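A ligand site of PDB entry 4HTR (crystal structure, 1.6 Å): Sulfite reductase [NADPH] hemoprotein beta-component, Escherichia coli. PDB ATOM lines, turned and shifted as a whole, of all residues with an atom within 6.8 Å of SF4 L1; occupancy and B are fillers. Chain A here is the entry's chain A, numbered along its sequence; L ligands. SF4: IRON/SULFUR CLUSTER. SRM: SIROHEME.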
ATOM      1  N   ALA A 370     -14.056  27.131 -27.017  1.00  0.00           N
ATOM      2  CA  ALA A 370     -15.476  27.440 -26.933  1.00  0.00           C
ATOM      3  C   ALA A 370     -16.278  26.489 -27.807  1.00  0.00           C
ATOM      4  O   ALA A 370     -15.776  25.905 -28.765  1.00  0.00           O
ATOM      5  CB  ALA A 370     -15.722  28.885 -27.369  1.00  0.00           C
ATOM      6  N   CYS A 371     -17.564  26.378 -27.497  1.00  0.00           N
ATOM      7  CA  CYS A 371     -18.489  25.647 -28.362  1.00  0.00           C
ATOM      8  C   CYS A 371     -19.014  26.555 -29.476  1.00  0.00           C
ATOM      9  O   CYS A 371     -18.818  27.787 -29.455  1.00  0.00           O
ATOM     10  CB  CYS A 371     -19.695  25.179 -27.547  1.00  0.00           C
ATOM     11  SG  CYS A 371     -20.804  26.534 -27.073  1.00  0.00           S
ATOM     12  N   VAL A 372     -19.720  25.960 -30.421  1.00  0.00           N
ATOM     13  CA  VAL A 372     -20.284  26.707 -31.550  1.00  0.00           C
ATOM     14  C   VAL A 372     -21.231  27.848 -31.127  1.00  0.00           C
ATOM     15  O   VAL A 372     -21.037  28.995 -31.538  1.00  0.00           O
ATOM     16  CB  VAL A 372     -21.023  25.758 -32.523  1.00  0.00           C
ATOM     17  CG1 VAL A 372     -21.736  26.550 -33.603  1.00  0.00           C
ATOM     18  CG2 VAL A 372     -20.037  24.767 -33.163  1.00  0.00           C
ATOM     19  N   SER A 373     -22.221  27.533 -30.289  1.00  0.00           N
ATOM     20  CA  SER A 373     -23.195  28.537 -29.838  1.00  0.00           C
ATOM     21  C   SER A 373     -23.803  29.269 -31.039  1.00  0.00           C
ATOM     22  O   SER A 373     -23.981  28.662 -32.102  1.00  0.00           O
ATOM     23  CB  SER A 373     -22.536  29.542 -28.888  1.00  0.00           C
ATOM     24  OG  SER A 373     -23.515  30.401 -28.303  1.00  0.00           O
ATOM     25  N   PHE A 374     -24.131  30.552 -30.879  1.00  0.00           N
ATOM     26  CA  PHE A 374     -24.627  31.379 -31.984  1.00  0.00           C
ATOM     27  C   PHE A 374     -23.583  31.414 -33.097  1.00  0.00           C
ATOM     28  O   PHE A 374     -22.374  31.388 -32.831  1.00  0.00           O
ATOM     29  CB  PHE A 374     -24.947  32.811 -31.510  1.00  0.00           C
ATOM     30  CG  PHE A 374     -25.992  32.888 -30.423  1.00  0.00           C
ATOM     31  CD1 PHE A 374     -27.329  32.625 -30.697  1.00  0.00           C
ATOM     32  CD2 PHE A 374     -25.645  33.272 -29.141  1.00  0.00           C
ATOM     33  CE1 PHE A 374     -28.296  32.716 -29.695  1.00  0.00           C
ATOM     34  CE2 PHE A 374     -26.600  33.363 -28.131  1.00  0.00           C
ATOM     35  CZ  PHE A 374     -27.930  33.094 -28.416  1.00  0.00           C
ATOM     36  N   CYS A 377     -26.504  27.394 -33.269  1.00  0.00           N
ATOM     37  CA  CYS A 377     -27.072  26.544 -32.230  1.00  0.00           C
ATOM     38  C   CYS A 377     -28.428  27.054 -31.742  1.00  0.00           C
ATOM     39  O   CYS A 377     -28.513  28.172 -31.249  1.00  0.00           O
ATOM     40  CB  CYS A 377     -26.127  26.398 -31.055  1.00  0.00           C
ATOM     41  SG  CYS A 377     -26.794  25.222 -29.869  1.00  0.00           S
ATOM     42  N   PRO A 378     -29.472  26.227 -31.864  1.00  0.00           N
ATOM     43  CA  PRO A 378     -30.796  26.687 -31.431  1.00  0.00           C
ATOM     44  C   PRO A 378     -30.947  26.739 -29.904  1.00  0.00           C
ATOM     45  O   PRO A 378     -31.920  27.294 -29.394  1.00  0.00           O
ATOM     46  CB  PRO A 378     -31.751  25.637 -32.026  1.00  0.00           C
ATOM     47  CG  PRO A 378     -30.914  24.390 -32.134  1.00  0.00           C
ATOM     48  CD  PRO A 378     -29.519  24.881 -32.471  1.00  0.00           C
ATOM     49  N   LEU A 379     -29.976  26.186 -29.182  1.00  0.00           N
ATOM     50  CA  LEU A 379     -30.072  26.131 -27.729  1.00  0.00           C
ATOM     51  C   LEU A 379     -29.234  27.205 -27.031  1.00  0.00           C
ATOM     52  O   LEU A 379     -29.226  27.313 -25.803  1.00  0.00           O
ATOM     53  CB  LEU A 379     -29.636  24.739 -27.233  1.00  0.00           C
ATOM     54  CG  LEU A 379     -30.204  23.551 -28.026  1.00  0.00           C
ATOM     55  CD1 LEU A 379     -29.698  22.203 -27.484  1.00  0.00           C
ATOM     56  CD2 LEU A 379     -31.735  23.591 -28.120  1.00  0.00           C
ATOM     57  N   ALA A 380     -28.504  28.003 -27.808  1.00  0.00           N
ATOM     58  CA  ALA A 380     -27.533  28.944 -27.257  1.00  0.00           C
ATOM     59  C   ALA A 380     -28.157  29.990 -26.347  1.00  0.00           C
ATOM     60  O   ALA A 380     -29.234  30.511 -26.640  1.00  0.00           O
ATOM     61  CB  ALA A 380     -26.746  29.610 -28.379  1.00  0.00           C
ATOM     62  N   MET A 381     -27.476  30.298 -25.251  1.00  0.00           N
ATOM     63  CA  MET A 381     -27.904  31.376 -24.361  1.00  0.00           C
ATOM     64  C   MET A 381     -26.975  32.573 -24.441  1.00  0.00           C
ATOM     65  O   MET A 381     -27.421  33.706 -24.379  1.00  0.00           O
ATOM     66  CB  MET A 381     -27.986  30.875 -22.917  1.00  0.00           C
ATOM     67  CG  MET A 381     -29.033  29.804 -22.724  1.00  0.00           C
ATOM     68  SD  MET A 381     -28.980  29.136 -21.051  1.00  0.00           S
ATOM     69  CE  MET A 381     -30.215  27.834 -21.162  1.00  0.00           C
ATOM     70  N   ALA A 382     -25.676  32.298 -24.575  1.00  0.00           N
ATOM     71  CA  ALA A 382     -24.703  33.372 -24.775  1.00  0.00           C
ATOM     72  C   ALA A 382     -23.696  32.975 -25.836  1.00  0.00           C
ATOM     73  O   ALA A 382     -23.467  31.778 -26.067  1.00  0.00           O
ATOM     74  CB  ALA A 382     -23.979  33.671 -23.470  1.00  0.00           C
ATOM     75  N   ALA A 384     -20.298  32.031 -27.669  1.00  0.00           N
ATOM     76  CA  ALA A 384     -19.152  31.254 -27.222  1.00  0.00           C
ATOM     77  C   ALA A 384     -18.058  31.359 -28.260  1.00  0.00           C
ATOM     78  O   ALA A 384     -17.135  32.148 -28.089  1.00  0.00           O
ATOM     79  CB  ALA A 384     -19.560  29.796 -26.965  1.00  0.00           C
ATOM     80  N   VAL A 413     -15.299  28.291 -22.743  1.00  0.00           N
ATOM     81  CA  VAL A 413     -16.591  28.992 -22.726  1.00  0.00           C
ATOM     82  C   VAL A 413     -17.616  28.129 -23.398  1.00  0.00           C
ATOM     83  O   VAL A 413     -17.411  27.675 -24.529  1.00  0.00           O
ATOM     84  CB  VAL A 413     -16.508  30.337 -23.500  1.00  0.00           C
ATOM     85  CG1 VAL A 413     -17.859  31.097 -23.426  1.00  0.00           C
ATOM     86  CG2 VAL A 413     -15.355  31.192 -22.970  1.00  0.00           C
ATOM     87  N   THR A 414     -18.714  27.863 -22.704  1.00  0.00           N
ATOM     88  CA  THR A 414     -19.783  27.070 -23.304  1.00  0.00           C
ATOM     89  C   THR A 414     -21.028  27.957 -23.347  1.00  0.00           C
ATOM     90  O   THR A 414     -21.280  28.728 -22.427  1.00  0.00           O
ATOM     91  CB  THR A 414     -19.969  25.708 -22.557  1.00  0.00           C
ATOM     92  OG1 THR A 414     -20.683  24.792 -23.396  1.00  0.00           O
ATOM     93  CG2 THR A 414     -20.715  25.893 -21.246  1.00  0.00           C
ATOM     94  N   GLY A 415     -21.754  27.895 -24.459  1.00  0.00           N
ATOM     95  CA  GLY A 415     -22.827  28.844 -24.720  1.00  0.00           C
ATOM     96  C   GLY A 415     -24.105  28.610 -23.944  1.00  0.00           C
ATOM     97  O   GLY A 415     -24.960  29.490 -23.864  1.00  0.00           O
ATOM     98  N   CYS A 416     -24.246  27.413 -23.399  1.00  0.00           N
ATOM     99  CA  CYS A 416     -25.373  27.115 -22.516  1.00  0.00           C
ATOM    100  C   CYS A 416     -24.938  25.956 -21.634  1.00  0.00           C
ATOM    101  O   CYS A 416     -23.836  25.420 -21.803  1.00  0.00           O
ATOM    102  CB  CYS A 416     -26.634  26.820 -23.321  1.00  0.00           C
ATOM    103  SG  CYS A 416     -26.751  25.147 -23.968  1.00  0.00           S
ATOM    104  N   PRO A 417     -25.784  25.549 -20.680  1.00  0.00           N
ATOM    105  CA  PRO A 417     -25.317  24.565 -19.690  1.00  0.00           C
ATOM    106  C   PRO A 417     -25.221  23.138 -20.214  1.00  0.00           C
ATOM    107  O   PRO A 417     -24.705  22.283 -19.490  1.00  0.00           O
ATOM    108  CB  PRO A 417     -26.361  24.672 -18.580  1.00  0.00           C
ATOM    109  CG  PRO A 417     -27.584  25.195 -19.228  1.00  0.00           C
ATOM    110  CD  PRO A 417     -27.100  26.107 -20.333  1.00  0.00           C
ATOM    111  N   ASN A 418     -25.680  22.883 -21.428  1.00  0.00           N
ATOM    112  CA  ASN A 418     -25.466  21.564 -22.023  1.00  0.00           C
ATOM    113  C   ASN A 418     -23.989  21.199 -22.016  1.00  0.00           C
ATOM    114  O   ASN A 418     -23.647  20.029 -21.893  1.00  0.00           O
ATOM    115  CB  ASN A 418     -26.043  21.526 -23.443  1.00  0.00           C
ATOM    116  CG  ASN A 418     -27.544  21.451 -23.443  1.00  0.00           C
ATOM    117  OD1 ASN A 418     -28.150  20.851 -22.552  1.00  0.00           O
ATOM    118  ND2 ASN A 418     -28.168  22.051 -24.447  1.00  0.00           N
ATOM    119  N   GLY A 419     -23.126  22.192 -22.155  1.00  0.00           N
ATOM    120  CA  GLY A 419     -21.722  22.037 -21.782  1.00  0.00           C
ATOM    121  C   GLY A 419     -20.758  21.536 -22.854  1.00  0.00           C
ATOM    122  O   GLY A 419     -19.666  21.055 -22.534  1.00  0.00           O
ATOM    123  N   CYS A 420     -21.160  21.676 -24.122  1.00  0.00           N
ATOM    124  CA  CYS A 420     -20.339  21.251 -25.263  1.00  0.00           C
ATOM    125  C   CYS A 420     -18.925  21.788 -25.287  1.00  0.00           C
ATOM    126  O   CYS A 420     -18.010  21.096 -25.762  1.00  0.00           O
ATOM    127  CB  CYS A 420     -21.019  21.668 -26.561  1.00  0.00           C
ATOM    128  SG  CYS A 420     -22.737  21.181 -26.661  1.00  0.00           S
ATOM    129  N   GLY A 421     -18.728  23.012 -24.791  1.00  0.00           N
ATOM    130  CA  GLY A 421     -17.406  23.611 -24.772  1.00  0.00           C
ATOM    131  C   GLY A 421     -16.508  22.994 -23.714  1.00  0.00           C
ATOM    132  O   GLY A 421     -15.342  23.354 -23.617  1.00  0.00           O
HETATM  133 FE1  SF4 L   1     -22.890  25.597 -26.950  1.00  0.00          FE
HETATM  134 FE2  SF4 L   1     -25.207  24.999 -28.301  1.00  0.00          FE
HETATM  135 FE3  SF4 L   1     -25.212  24.966 -25.588  1.00  0.00          FE
HETATM  136 FE4  SF4 L   1     -23.759  23.115 -26.982  1.00  0.00          FE
HETATM  137  S1  SF4 L   1     -25.914  23.375 -26.962  1.00  0.00           S
HETATM  138  S2  SF4 L   1     -23.151  24.292 -25.197  1.00  0.00           S
HETATM  139  S3  SF4 L   1     -23.163  24.313 -28.739  1.00  0.00           S
HETATM  140  S4  SF4 L   1     -24.784  26.672 -26.926  1.00  0.00           S
HETATM  141 FE   SRM L   2     -22.965  19.132 -28.031  1.00  0.00          FE
HETATM  142  CHA SRM L   2     -26.323  19.542 -28.264  1.00  0.00           C
HETATM  143  CHB SRM L   2     -22.473  21.211 -30.640  1.00  0.00           C
HETATM  144  CHC SRM L   2     -19.690  18.363 -28.050  1.00  0.00           C
HETATM  145  CHD SRM L   2     -23.250  18.126 -24.826  1.00  0.00           C
HETATM  146  NA  SRM L   2     -24.171  20.120 -29.241  1.00  0.00           N
HETATM  147  C1A SRM L   2     -25.540  20.105 -29.255  1.00  0.00           C
HETATM  148  C2A SRM L   2     -26.081  20.676 -30.547  1.00  0.00           C
HETATM  149  CMA SRM L   2     -26.300  19.554 -31.575  1.00  0.00           C
HETATM  150  CDA SRM L   2     -27.354  21.503 -30.329  1.00  0.00           C
HETATM  151  CEA SRM L   2     -28.633  20.716 -30.586  1.00  0.00           C
HETATM  152  O3A SRM L   2     -28.985  19.761 -29.860  1.00  0.00           O
HETATM  153  O4A SRM L   2     -29.369  21.022 -31.546  1.00  0.00           O
HETATM  154  C3A SRM L   2     -24.938  21.547 -30.943  1.00  0.00           C
HETATM  155  CAA SRM L   2     -24.943  22.031 -32.374  1.00  0.00           C
HETATM  156  CBA SRM L   2     -24.326  23.438 -32.423  1.00  0.00           C
HETATM  157  CCA SRM L   2     -24.053  23.832 -33.851  1.00  0.00           C
HETATM  158  O1A SRM L   2     -24.786  24.675 -34.429  1.00  0.00           O
HETATM  159  O2A SRM L   2     -23.090  23.325 -34.472  1.00  0.00           O
HETATM  160  C4A SRM L   2     -23.776  20.966 -30.230  1.00  0.00           C
HETATM  161  NB  SRM L   2     -21.430  19.603 -29.174  1.00  0.00           N
HETATM  162  C1B SRM L   2     -21.370  20.524 -30.159  1.00  0.00           C
HETATM  163  C2B SRM L   2     -19.958  20.681 -30.671  1.00  0.00           C
HETATM  164  CMB SRM L   2     -19.982  20.987 -32.180  1.00  0.00           C
HETATM  165  CDB SRM L   2     -19.198  21.779 -29.901  1.00  0.00           C
HETATM  166  CEB SRM L   2     -17.924  22.305 -30.545  1.00  0.00           C
HETATM  167  O3B SRM L   2     -17.802  23.522 -30.760  1.00  0.00           O
HETATM  168  O4B SRM L   2     -16.961  21.571 -30.866  1.00  0.00           O
HETATM  169  C3B SRM L   2     -19.463  19.291 -30.392  1.00  0.00           C
HETATM  170  CAB SRM L   2     -19.698  18.351 -31.561  1.00  0.00           C
HETATM  171  CBB SRM L   2     -19.131  16.995 -31.115  1.00  0.00           C
HETATM  172  CCB SRM L   2     -19.285  15.926 -32.163  1.00  0.00           C
HETATM  173  O1B SRM L   2     -18.643  16.003 -33.225  1.00  0.00           O
HETATM  174  O2B SRM L   2     -20.039  14.932 -31.982  1.00  0.00           O
HETATM  175  C4B SRM L   2     -20.191  19.051 -29.120  1.00  0.00           C
HETATM  176  NC  SRM L   2     -21.718  18.414 -26.692  1.00  0.00           N
HETATM  177  C1C SRM L   2     -20.393  18.179 -26.876  1.00  0.00           C
HETATM  178  C2C SRM L   2     -19.734  17.677 -25.643  1.00  0.00           C
HETATM  179  CDC SRM L   2     -18.256  17.645 -25.389  1.00  0.00           C
HETATM  180  CEC SRM L   2     -17.752  16.271 -25.792  1.00  0.00           C
HETATM  181  O3C SRM L   2     -18.556  15.365 -26.080  1.00  0.00           O
HETATM  182  O4C SRM L   2     -16.531  16.050 -25.831  1.00  0.00           O
HETATM  183  C3C SRM L   2     -20.760  17.806 -24.609  1.00  0.00           C
HETATM  184  CAC SRM L   2     -20.572  17.739 -23.115  1.00  0.00           C
HETATM  185  CBC SRM L   2     -20.239  16.305 -22.681  1.00  0.00           C
HETATM  186  CCC SRM L   2     -21.504  15.513 -22.446  1.00  0.00           C
HETATM  187  O1C SRM L   2     -22.097  14.944 -23.390  1.00  0.00           O
HETATM  188  O2C SRM L   2     -21.976  15.406 -21.292  1.00  0.00           O
HETATM  189  C4C SRM L   2     -21.986  18.124 -25.394  1.00  0.00           C
HETATM  190  ND  SRM L   2     -24.488  18.755 -26.835  1.00  0.00           N
HETATM  191  C1D SRM L   2     -24.403  18.406 -25.518  1.00  0.00           C
HETATM  192  C2D SRM L   2     -25.740  18.283 -24.894  1.00  0.00           C
HETATM  193  CAD SRM L   2     -26.070  17.843 -23.481  1.00  0.00           C
HETATM  194  CBD SRM L   2     -26.485  16.374 -23.519  1.00  0.00           C
HETATM  195  CCD SRM L   2     -26.767  15.921 -22.112  1.00  0.00           C
HETATM  196  O1D SRM L   2     -26.091  14.986 -21.611  1.00  0.00           O
HETATM  197  O2D SRM L   2     -27.672  16.464 -21.441  1.00  0.00           O
HETATM  198  C3D SRM L   2     -26.660  18.742 -25.919  1.00  0.00           C
HETATM  199  CDD SRM L   2     -28.147  18.950 -25.798  1.00  0.00           C
HETATM  200  CED SRM L   2     -28.958  17.730 -26.165  1.00  0.00           C
HETATM  201  O3D SRM L   2     -28.412  16.704 -26.636  1.00  0.00           O
HETATM  202  O4D SRM L   2     -30.202  17.750 -26.004  1.00  0.00           O
HETATM  203  C4D SRM L   2     -25.801  19.029 -27.095  1.00  0.00           C
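A sulfur (S2) of SF4 L1 lies close to the side-chain hydroxyl (OG1) of Thr 414, at 3.1 Å.
S1 of SF4 L1 sits close to ND2 of Asn 418 (3.6 Å).
The side-chain sulfur (SG) of Cys 371 binds an iron atom (FE1) of SF4 L1, 2.3 Å away.
An oxygen (O1A) of SRM L2 lies within hydrogen-bond range of the backbone NH of Cys 377 (3.4 Å).
The backbone NH of Cys 416 lies close to a sulfur (S4) of SF4 L1 (3.6 Å).
An iron atom (FE4) of SF4 L1 is bound by the side-chain sulfur of Cys 420, at 2.2 Å.
S2 of SF4 L1 sits close to N of Gly 419 (3.7 Å).
FE of SRM L2 is bound by SG of Cys 420.
The backbone NH of Cys 420 lies close to a sulfur (S2) of SF4 L1 (3.5 Å).
N of Ser 373 sits close to S3 of SF4 L1, 3.7 Å away.
The side-chain sulfur of Cys 377 binds an iron atom (FE2) of SF4 L1 (2.2 Å).
N of Val 372 lies within hydrogen-bond range of O3B of SRM L2, 3.1 Å away.
FE3 of SF4 L1 is bound by SG of Cys 416 (2.2 Å).
Leu 379 touches SF4 L1.
Ala 380 touches SF4 L1 (CA to S4, 3.6 Å).
Gly 415 touches SF4 L1.
Hydrophobic or aromatic side chains within 4 Å of SF4 L1: Leu 379 and Ala 380.
11 residues have an atom within 4 Å of SF4 L1: Cys 371, Ser 373, Cys 377, Leu 379, Ala 380, Thr 414, Gly 415, Cys 416, Asn 418, Gly 419 and Cys 420.
The backbone carbonyl oxygen of Val 413 lies within hydrogen-bond range of the backbone NH of Cys 371 (3.2 Å).
SG of Cys 371 lies close to N of Gly 415, at 3.1 Å.
N of Met 381 is in hydrogen-bond range of O of Gly 415 (3.0 Å).
SG of Cys 377 sits close to N of Leu 379 (3.4 Å).
OG of Ser 373 sits at hydrogen-bond distance from O of Ala 382 (2.6 Å).
The side-chain amide nitrogen of Asn 418 lies close to the side-chain sulfur of Cys 416 (3.4 Å).
The backbone carbonyl oxygen (O) of Gly 415 sits at hydrogen-bond distance from the backbone NH (N) of Ala 382 (3.0 Å).
The side-chain sulfur of Cys 416 lies close to the backbone carbonyl oxygen of Leu 379.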
